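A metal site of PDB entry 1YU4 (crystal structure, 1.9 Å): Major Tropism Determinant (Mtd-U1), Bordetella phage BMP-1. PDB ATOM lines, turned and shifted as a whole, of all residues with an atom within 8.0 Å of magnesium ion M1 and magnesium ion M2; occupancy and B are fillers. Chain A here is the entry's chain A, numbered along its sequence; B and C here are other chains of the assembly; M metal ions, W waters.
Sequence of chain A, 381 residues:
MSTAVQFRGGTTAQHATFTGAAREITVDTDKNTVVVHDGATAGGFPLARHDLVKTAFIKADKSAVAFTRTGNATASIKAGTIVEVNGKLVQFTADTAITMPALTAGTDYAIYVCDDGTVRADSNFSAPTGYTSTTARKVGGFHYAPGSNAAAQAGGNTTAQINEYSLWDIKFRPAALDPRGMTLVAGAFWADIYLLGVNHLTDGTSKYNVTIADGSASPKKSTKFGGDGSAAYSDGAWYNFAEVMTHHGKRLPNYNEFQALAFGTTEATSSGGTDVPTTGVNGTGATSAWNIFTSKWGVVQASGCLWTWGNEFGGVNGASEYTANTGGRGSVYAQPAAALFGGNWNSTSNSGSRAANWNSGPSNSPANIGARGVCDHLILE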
ATOM      1  N   ASN A 254      -4.658  -9.396 -21.755  1.00  0.00           N
ATOM      2  CA  ASN A 254      -5.917  -8.806 -22.146  1.00  0.00           C
ATOM      3  C   ASN A 254      -6.749  -9.889 -22.806  1.00  0.00           C
ATOM      4  O   ASN A 254      -6.321 -11.037 -22.908  1.00  0.00           O
ATOM      5  CB  ASN A 254      -5.690  -7.601 -23.066  1.00  0.00           C
ATOM      6  CG  ASN A 254      -6.669  -6.461 -22.793  1.00  0.00           C
ATOM      7  OD1 ASN A 254      -7.887  -6.637 -22.867  1.00  0.00           O
ATOM      8  ND2 ASN A 254      -6.141  -5.293 -22.482  1.00  0.00           N
ATOM      9  N   ASN A 311      -5.454  -7.647 -17.682  1.00  0.00           N
ATOM     10  CA  ASN A 311      -4.948  -6.269 -17.704  1.00  0.00           C
ATOM     11  C   ASN A 311      -5.938  -5.337 -18.418  1.00  0.00           C
ATOM     12  O   ASN A 311      -5.575  -4.564 -19.298  1.00  0.00           O
ATOM     13  CB  ASN A 311      -3.556  -6.238 -18.358  1.00  0.00           C
ATOM     14  CG  ASN A 311      -2.825  -4.940 -18.125  1.00  0.00           C
ATOM     15  OD1 ASN A 311      -2.683  -4.476 -16.981  1.00  0.00           O
ATOM     16  ND2 ASN A 311      -2.335  -4.345 -19.217  1.00  0.00           N
ATOM     17  N   GLU A 312      -7.195  -5.431 -18.002  1.00  0.00           N
ATOM     18  CA  GLU A 312      -8.270  -4.673 -18.627  1.00  0.00           C
ATOM     19  C   GLU A 312      -9.403  -4.506 -17.633  1.00  0.00           C
ATOM     20  O   GLU A 312      -9.735  -5.421 -16.879  1.00  0.00           O
ATOM     21  CB  GLU A 312      -8.752  -5.409 -19.884  1.00  0.00           C
ATOM     22  CG  GLU A 312      -9.922  -4.758 -20.625  1.00  0.00           C
ATOM     23  CD  GLU A 312      -9.580  -3.415 -21.227  1.00  0.00           C
ATOM     24  OE1 GLU A 312      -8.387  -3.131 -21.455  1.00  0.00           O
ATOM     25  OE2 GLU A 312     -10.504  -2.630 -21.478  1.00  0.00           O
ATOM     26  N   PHE A 313     -10.002  -3.316 -17.658  1.00  0.00           N
ATOM     27  CA  PHE A 313     -11.058  -2.947 -16.729  1.00  0.00           C
ATOM     28  C   PHE A 313     -12.355  -2.637 -17.470  1.00  0.00           C
ATOM     29  O   PHE A 313     -12.350  -2.118 -18.594  1.00  0.00           O
ATOM     30  CB  PHE A 313     -10.609  -1.738 -15.908  1.00  0.00           C
ATOM     31  CG  PHE A 313      -9.503  -2.044 -14.952  1.00  0.00           C
ATOM     32  CD1 PHE A 313      -9.785  -2.368 -13.635  1.00  0.00           C
ATOM     33  CD2 PHE A 313      -8.179  -2.048 -15.373  1.00  0.00           C
ATOM     34  CE1 PHE A 313      -8.769  -2.670 -12.742  1.00  0.00           C
ATOM     35  CE2 PHE A 313      -7.158  -2.358 -14.491  1.00  0.00           C
ATOM     36  CZ  PHE A 313      -7.448  -2.671 -13.176  1.00  0.00           C
ATOM     37  N   GLY A 314     -13.470  -2.962 -16.816  1.00  0.00           N
ATOM     38  CA  GLY A 314     -14.802  -2.763 -17.353  1.00  0.00           C
ATOM     39  C   GLY A 314     -15.811  -3.620 -16.617  1.00  0.00           C
ATOM     40  O   GLY A 314     -15.455  -4.390 -15.714  1.00  0.00           O
ATOM     41  N   GLY A 315     -17.071  -3.522 -17.006  1.00  0.00           N
ATOM     42  CA  GLY A 315     -18.123  -4.289 -16.374  1.00  0.00           C
ATOM     43  C   GLY A 315     -18.710  -3.589 -15.161  1.00  0.00           C
ATOM     44  O   GLY A 315     -18.932  -2.375 -15.173  1.00  0.00           O
ATOM     45  N   PRO A 336     -14.149   0.194 -11.820  1.00  0.00           N
ATOM     46  CA  PRO A 336     -14.595  -0.950 -12.620  1.00  0.00           C
ATOM     47  C   PRO A 336     -13.901  -2.251 -12.233  1.00  0.00           C
ATOM     48  O   PRO A 336     -12.757  -2.249 -11.740  1.00  0.00           O
ATOM     49  CB  PRO A 336     -14.215  -0.539 -14.041  1.00  0.00           C
ATOM     50  CG  PRO A 336     -13.088   0.381 -13.872  1.00  0.00           C
ATOM     51  CD  PRO A 336     -13.385   1.156 -12.626  1.00  0.00           C
ATOM     52  N   ALA A 337     -14.589  -3.357 -12.484  1.00  0.00           N
ATOM     53  CA  ALA A 337     -14.003  -4.677 -12.315  1.00  0.00           C
ATOM     54  C   ALA A 337     -12.745  -4.813 -13.158  1.00  0.00           C
ATOM     55  O   ALA A 337     -12.611  -4.184 -14.209  1.00  0.00           O
ATOM     56  CB  ALA A 337     -15.006  -5.773 -12.709  1.00  0.00           C
ATOM     57  N   TRP A 358     -16.620 -10.096 -15.335  1.00  0.00           N
ATOM     58  CA  TRP A 358     -16.303  -8.686 -15.085  1.00  0.00           C
ATOM     59  C   TRP A 358     -17.119  -8.164 -13.918  1.00  0.00           C
ATOM     60  O   TRP A 358     -17.638  -7.046 -13.960  1.00  0.00           O
ATOM     61  CB  TRP A 358     -16.571  -7.834 -16.326  1.00  0.00           C
ATOM     62  CG  TRP A 358     -15.946  -8.337 -17.583  1.00  0.00           C
ATOM     63  CD1 TRP A 358     -16.333  -9.411 -18.328  1.00  0.00           C
ATOM     64  CD2 TRP A 358     -14.857  -7.738 -18.289  1.00  0.00           C
ATOM     65  NE1 TRP A 358     -15.549  -9.522 -19.442  1.00  0.00           N
ATOM     66  CE2 TRP A 358     -14.634  -8.507 -19.454  1.00  0.00           C
ATOM     67  CE3 TRP A 358     -14.043  -6.618 -18.067  1.00  0.00           C
ATOM     68  CZ2 TRP A 358     -13.638  -8.199 -20.376  1.00  0.00           C
ATOM     69  CZ3 TRP A 358     -13.060  -6.320 -18.989  1.00  0.00           C
ATOM     70  CH2 TRP A 358     -12.859  -7.108 -20.131  1.00  0.00           C
ATOM     71  N   ASN B 254      -1.409   2.918 -17.862  1.00  0.00           N
ATOM     72  CA  ASN B 254      -2.497   2.097 -17.382  1.00  0.00           C
ATOM     73  C   ASN B 254      -2.327   1.889 -15.876  1.00  0.00           C
ATOM     74  O   ASN B 254      -1.357   2.370 -15.295  1.00  0.00           O
ATOM     75  CB  ASN B 254      -2.544   0.759 -18.126  1.00  0.00           C
ATOM     76  CG  ASN B 254      -3.953   0.300 -18.389  1.00  0.00           C
ATOM     77  OD1 ASN B 254      -4.738   0.152 -17.465  1.00  0.00           O
ATOM     78  ND2 ASN B 254      -4.289   0.082 -19.655  1.00  0.00           N
ATOM     79  N   ASN B 311      -4.540   5.446 -19.767  1.00  0.00           N
ATOM     80  CA  ASN B 311      -4.811   4.887 -21.084  1.00  0.00           C
ATOM     81  C   ASN B 311      -5.736   3.670 -20.959  1.00  0.00           C
ATOM     82  O   ASN B 311      -5.408   2.575 -21.421  1.00  0.00           O
ATOM     83  CB  ASN B 311      -3.491   4.493 -21.760  1.00  0.00           C
ATOM     84  CG  ASN B 311      -3.669   4.152 -23.223  1.00  0.00           C
ATOM     85  OD1 ASN B 311      -4.266   4.922 -23.976  1.00  0.00           O
ATOM     86  ND2 ASN B 311      -3.174   2.989 -23.629  1.00  0.00           N
ATOM     87  N   GLU B 312      -6.875   3.879 -20.323  1.00  0.00           N
ATOM     88  CA  GLU B 312      -7.800   2.805 -19.997  1.00  0.00           C
ATOM     89  C   GLU B 312      -9.167   3.404 -19.702  1.00  0.00           C
ATOM     90  O   GLU B 312      -9.279   4.466 -19.076  1.00  0.00           O
ATOM     91  CB  GLU B 312      -7.292   2.017 -18.781  1.00  0.00           C
ATOM     92  CG  GLU B 312      -8.173   0.880 -18.294  1.00  0.00           C
ATOM     93  CD  GLU B 312      -8.371  -0.245 -19.286  1.00  0.00           C
ATOM     94  OE1 GLU B 312      -7.507  -0.464 -20.174  1.00  0.00           O
ATOM     95  OE2 GLU B 312      -9.409  -0.927 -19.191  1.00  0.00           O
ATOM     96  N   PHE B 313     -10.203   2.725 -20.174  1.00  0.00           N
ATOM     97  CA  PHE B 313     -11.576   3.190 -20.032  1.00  0.00           C
ATOM     98  C   PHE B 313     -12.423   2.203 -19.223  1.00  0.00           C
ATOM     99  O   PHE B 313     -12.198   1.003 -19.260  1.00  0.00           O
ATOM    100  CB  PHE B 313     -12.185   3.441 -21.413  1.00  0.00           C
ATOM    101  CG  PHE B 313     -11.551   4.589 -22.153  1.00  0.00           C
ATOM    102  CD1 PHE B 313     -12.130   5.849 -22.144  1.00  0.00           C
ATOM    103  CD2 PHE B 313     -10.363   4.409 -22.844  1.00  0.00           C
ATOM    104  CE1 PHE B 313     -11.546   6.923 -22.823  1.00  0.00           C
ATOM    105  CE2 PHE B 313      -9.761   5.477 -23.528  1.00  0.00           C
ATOM    106  CZ  PHE B 313     -10.354   6.727 -23.519  1.00  0.00           C
ATOM    107  N   GLY B 314     -13.404   2.755 -18.512  1.00  0.00           N
ATOM    108  CA  GLY B 314     -14.264   2.002 -17.619  1.00  0.00           C
ATOM    109  C   GLY B 314     -14.868   2.930 -16.573  1.00  0.00           C
ATOM    110  O   GLY B 314     -14.553   4.122 -16.526  1.00  0.00           O
ATOM    111  N   GLY B 315     -15.747   2.383 -15.742  1.00  0.00           N
ATOM    112  CA  GLY B 315     -16.423   3.166 -14.722  1.00  0.00           C
ATOM    113  C   GLY B 315     -17.714   3.804 -15.207  1.00  0.00           C
ATOM    114  O   GLY B 315     -18.505   3.167 -15.909  1.00  0.00           O
ATOM    115  N   PRO B 336     -17.491   5.551 -21.867  1.00  0.00           N
ATOM    116  CA  PRO B 336     -16.961   5.349 -20.518  1.00  0.00           C
ATOM    117  C   PRO B 336     -15.947   6.409 -20.120  1.00  0.00           C
ATOM    118  O   PRO B 336     -15.302   7.027 -20.978  1.00  0.00           O
ATOM    119  CB  PRO B 336     -16.274   3.988 -20.614  1.00  0.00           C
ATOM    120  CG  PRO B 336     -15.902   3.868 -22.055  1.00  0.00           C
ATOM    121  CD  PRO B 336     -17.029   4.509 -22.784  1.00  0.00           C
ATOM    122  N   ALA B 337     -15.789   6.577 -18.815  1.00  0.00           N
ATOM    123  CA  ALA B 337     -14.754   7.442 -18.273  1.00  0.00           C
ATOM    124  C   ALA B 337     -13.379   6.926 -18.677  1.00  0.00           C
ATOM    125  O   ALA B 337     -13.187   5.724 -18.877  1.00  0.00           O
ATOM    126  CB  ALA B 337     -14.849   7.484 -16.756  1.00  0.00           C
ATOM    127  N   TRP B 358     -12.819   6.999 -11.751  1.00  0.00           N
ATOM    128  CA  TRP B 358     -13.397   6.603 -13.031  1.00  0.00           C
ATOM    129  C   TRP B 358     -14.743   7.288 -13.252  1.00  0.00           C
ATOM    130  O   TRP B 358     -15.691   6.675 -13.756  1.00  0.00           O
ATOM    131  CB  TRP B 358     -13.544   5.087 -13.125  1.00  0.00           C
ATOM    132  CG  TRP B 358     -12.310   4.287 -12.790  1.00  0.00           C
ATOM    133  CD1 TRP B 358     -11.790   4.044 -11.552  1.00  0.00           C
ATOM    134  CD2 TRP B 358     -11.464   3.580 -13.708  1.00  0.00           C
ATOM    135  NE1 TRP B 358     -10.677   3.245 -11.636  1.00  0.00           N
ATOM    136  CE2 TRP B 358     -10.458   2.947 -12.954  1.00  0.00           C
ATOM    137  CE3 TRP B 358     -11.461   3.415 -15.102  1.00  0.00           C
ATOM    138  CZ2 TRP B 358      -9.459   2.174 -13.540  1.00  0.00           C
ATOM    139  CZ3 TRP B 358     -10.472   2.636 -15.681  1.00  0.00           C
ATOM    140  CH2 TRP B 358      -9.483   2.027 -14.895  1.00  0.00           C
ATOM    141  N   ASN C 254      -6.584   0.860 -29.909  1.00  0.00           N
ATOM    142  CA  ASN C 254      -7.192   1.508 -28.755  1.00  0.00           C
ATOM    143  C   ASN C 254      -7.564   2.948 -29.153  1.00  0.00           C
ATOM    144  O   ASN C 254      -7.300   3.361 -30.277  1.00  0.00           O
ATOM    145  CB  ASN C 254      -6.258   1.483 -27.557  1.00  0.00           C
ATOM    146  CG  ASN C 254      -7.007   1.281 -26.269  1.00  0.00           C
ATOM    147  OD1 ASN C 254      -7.917   2.041 -25.945  1.00  0.00           O
ATOM    148  ND2 ASN C 254      -6.650   0.234 -25.531  1.00  0.00           N
ATOM    149  N   ASN C 311      -9.464  -2.489 -29.301  1.00  0.00           N
ATOM    150  CA  ASN C 311      -8.866  -3.387 -28.312  1.00  0.00           C
ATOM    151  C   ASN C 311      -9.037  -2.840 -26.897  1.00  0.00           C
ATOM    152  O   ASN C 311      -8.094  -2.751 -26.124  1.00  0.00           O
ATOM    153  CB  ASN C 311      -7.383  -3.600 -28.618  1.00  0.00           C
ATOM    154  CG  ASN C 311      -6.801  -4.795 -27.875  1.00  0.00           C
ATOM    155  OD1 ASN C 311      -7.389  -5.879 -27.854  1.00  0.00           O
ATOM    156  ND2 ASN C 311      -5.641  -4.606 -27.256  1.00  0.00           N
ATOM    157  N   GLU C 312     -10.271  -2.468 -26.567  1.00  0.00           N
ATOM    158  CA  GLU C 312     -10.592  -1.824 -25.300  1.00  0.00           C
ATOM    159  C   GLU C 312     -12.050  -2.048 -24.962  1.00  0.00           C
ATOM    160  O   GLU C 312     -12.917  -2.041 -25.846  1.00  0.00           O
ATOM    161  CB  GLU C 312     -10.284  -0.319 -25.403  1.00  0.00           C
ATOM    162  CG  GLU C 312     -10.623   0.494 -24.161  1.00  0.00           C
ATOM    163  CD  GLU C 312      -9.787   0.137 -22.943  1.00  0.00           C
ATOM    164  OE1 GLU C 312      -8.679  -0.418 -23.083  1.00  0.00           O
ATOM    165  OE2 GLU C 312     -10.247   0.421 -21.825  1.00  0.00           O
ATOM    166  N   PHE C 313     -12.310  -2.267 -23.685  1.00  0.00           N
ATOM    167  CA  PHE C 313     -13.642  -2.617 -23.208  1.00  0.00           C
ATOM    168  C   PHE C 313     -14.165  -1.596 -22.210  1.00  0.00           C
ATOM    169  O   PHE C 313     -13.400  -1.064 -21.400  1.00  0.00           O
ATOM    170  CB  PHE C 313     -13.615  -4.009 -22.578  1.00  0.00           C
ATOM    171  CG  PHE C 313     -13.444  -5.109 -23.592  1.00  0.00           C
ATOM    172  CD1 PHE C 313     -14.551  -5.761 -24.125  1.00  0.00           C
ATOM    173  CD2 PHE C 313     -12.172  -5.488 -24.012  1.00  0.00           C
ATOM    174  CE1 PHE C 313     -14.392  -6.754 -25.062  1.00  0.00           C
ATOM    175  CE2 PHE C 313     -12.016  -6.487 -24.957  1.00  0.00           C
ATOM    176  CZ  PHE C 313     -13.116  -7.121 -25.480  1.00  0.00           C
ATOM    177  N   GLY C 314     -15.460  -1.321 -22.287  1.00  0.00           N
ATOM    178  CA  GLY C 314     -16.130  -0.426 -21.369  1.00  0.00           C
ATOM    179  C   GLY C 314     -17.482  -0.015 -21.907  1.00  0.00           C
ATOM    180  O   GLY C 314     -17.893  -0.482 -22.962  1.00  0.00           O
ATOM    181  N   GLY C 315     -18.181   0.871 -21.213  1.00  0.00           N
ATOM    182  CA  GLY C 315     -19.492   1.327 -21.646  1.00  0.00           C
ATOM    183  C   GLY C 315     -20.613   0.405 -21.175  1.00  0.00           C
ATOM    184  O   GLY C 315     -20.641  -0.034 -20.028  1.00  0.00           O
ATOM    185  N   PRO C 336     -18.551  -6.175 -20.711  1.00  0.00           N
ATOM    186  CA  PRO C 336     -18.589  -4.813 -21.265  1.00  0.00           C
ATOM    187  C   PRO C 336     -18.535  -4.801 -22.798  1.00  0.00           C
ATOM    188  O   PRO C 336     -17.968  -5.712 -23.428  1.00  0.00           O
ATOM    189  CB  PRO C 336     -17.330  -4.169 -20.681  1.00  0.00           C
ATOM    190  CG  PRO C 336     -16.409  -5.326 -20.416  1.00  0.00           C
ATOM    191  CD  PRO C 336     -17.305  -6.435 -19.979  1.00  0.00           C
ATOM    192  N   ALA C 337     -19.105  -3.761 -23.393  1.00  0.00           N
ATOM    193  CA  ALA C 337     -18.946  -3.529 -24.825  1.00  0.00           C
ATOM    194  C   ALA C 337     -17.475  -3.487 -25.191  1.00  0.00           C
ATOM    195  O   ALA C 337     -16.625  -3.136 -24.379  1.00  0.00           O
ATOM    196  CB  ALA C 337     -19.626  -2.228 -25.245  1.00  0.00           C
ATOM    197  N   TRP C 358     -19.897   2.650 -27.570  1.00  0.00           N
ATOM    198  CA  TRP C 358     -19.581   1.649 -26.548  1.00  0.00           C
ATOM    199  C   TRP C 358     -20.856   0.882 -26.145  1.00  0.00           C
ATOM    200  O   TRP C 358     -21.068   0.565 -24.980  1.00  0.00           O
ATOM    201  CB  TRP C 358     -18.932   2.304 -25.342  1.00  0.00           C
ATOM    202  CG  TRP C 358     -17.689   3.089 -25.639  1.00  0.00           C
ATOM    203  CD1 TRP C 358     -17.638   4.340 -26.213  1.00  0.00           C
ATOM    204  CD2 TRP C 358     -16.338   2.718 -25.358  1.00  0.00           C
ATOM    205  NE1 TRP C 358     -16.331   4.747 -26.318  1.00  0.00           N
ATOM    206  CE2 TRP C 358     -15.517   3.783 -25.783  1.00  0.00           C
ATOM    207  CE3 TRP C 358     -15.737   1.587 -24.781  1.00  0.00           C
ATOM    208  CZ2 TRP C 358     -14.122   3.754 -25.656  1.00  0.00           C
ATOM    209  CZ3 TRP C 358     -14.351   1.561 -24.652  1.00  0.00           C
ATOM    210  CH2 TRP C 358     -13.563   2.640 -25.097  1.00  0.00           C
HETATM  211 MG    MG M   1     -11.415  -0.888 -20.258  1.00  0.00          MG
HETATM  212 MG    MG M   2      -7.176  -1.432 -21.964  1.00  0.00          MG
HETATM  213  O   HOH W   1      -5.763   0.053 -22.477  1.00  0.00           O
HETATM  214  O   HOH W   2      -5.622  -2.534 -21.080  1.00  0.00           O
HETATM  215  O   HOH W   3      -6.655  -2.402 -23.931  1.00  0.00           O
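ND2 of Asn 254 of chain B sits close to OE1 of Glu 312 of chain B (3.3 Å).
ND2 of Asn 254 of chain C lies close to OE1 of Glu 312 of chain C.
OE1 of Glu 312 of chain A sits close to ND2 of Asn 254 of chain A, 3.3 Å away.
ND2 of Asn 254 of chain C sits at hydrogen-bond distance from O of Asn 311 of chain C (3.4 Å).
The backbone carbonyl oxygen (O) of Asn 311 of chain B sits at hydrogen-bond distance from the side-chain amide nitrogen (ND2) of Asn 254 of chain B (3.3 Å).
Six residues have an atom within 4 Å of magnesium ion M1: Glu 312 of chain A, Phe 313 of chain A, Glu 312 of chain B, Phe 313 of chain B, Glu 312 of chain C and Phe 313 of chain C.
Merely in contact with magnesium ion M2: Asn 254 of chain C (3.97 Å) and Asn 254 of chain B (3.99 Å).
Within 4 Å of magnesium ion M2: Glu 312 of chain A, Asn 254 of chain B, Glu 312 of chain B, Asn 254 of chain C and Glu 312 of chain C.
The nearest printed residue that does not touch magnesium ion M2 is Asn 254 of chain A (4.03 Å).
Magnesium ion M1 is bound by O of Phe 313 of chain A (2.3 Å), OE2 of Glu 312 of chain B (2.3 Å), O of Phe 313 of chain B (2.3 Å), O of Phe 313 of chain C (2.3 Å), OE2 of Glu 312 of chain A (2.3 Å) and OE2 of Glu 312 of chain C (2.4 Å).
OE1 of Glu 312 of chain B binds magnesium ion M2 (2.1 Å).
Water W2 is bound to magnesium ion M2, at 2.1 Å.
Magnesium ion M2 is bound by water W1 (2.1 Å).
The side-chain carboxylate (OE1) of Glu 312 of chain C is bound to magnesium ion M2 (2.1 Å).
Magnesium ion M2 is bound by the side-chain carboxylate (OE1) of Glu 312 of chain A.
Water W3 is bound to magnesium ion M2, at 2.3 Å.
Magnesium ion M2 has six donor atoms within binding distance.
Water W1 lies within hydrogen-bond range of the backbone carbonyl oxygen (O) of Asn 311 of chain B (2.8 Å), the side-chain amide nitrogen (ND2) of Asn 254 of chain C (3.2 Å) and the side-chain amide nitrogen (ND2) of Asn 254 of chain B (3.2 Å).
Water W2 lies within hydrogen-bond range of the backbone carbonyl oxygen of Asn 311 of chain A (2.7 Å), the side-chain amide nitrogen of Asn 254 of chain A (3.1 Å) and the side-chain amide nitrogen of Asn 254 of chain B (3.3 Å).
Water W3 lies within hydrogen-bond range of O of Asn 311 of chain C, ND2 of Asn 254 of chain C and ND2 of Asn 254 of chain A.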
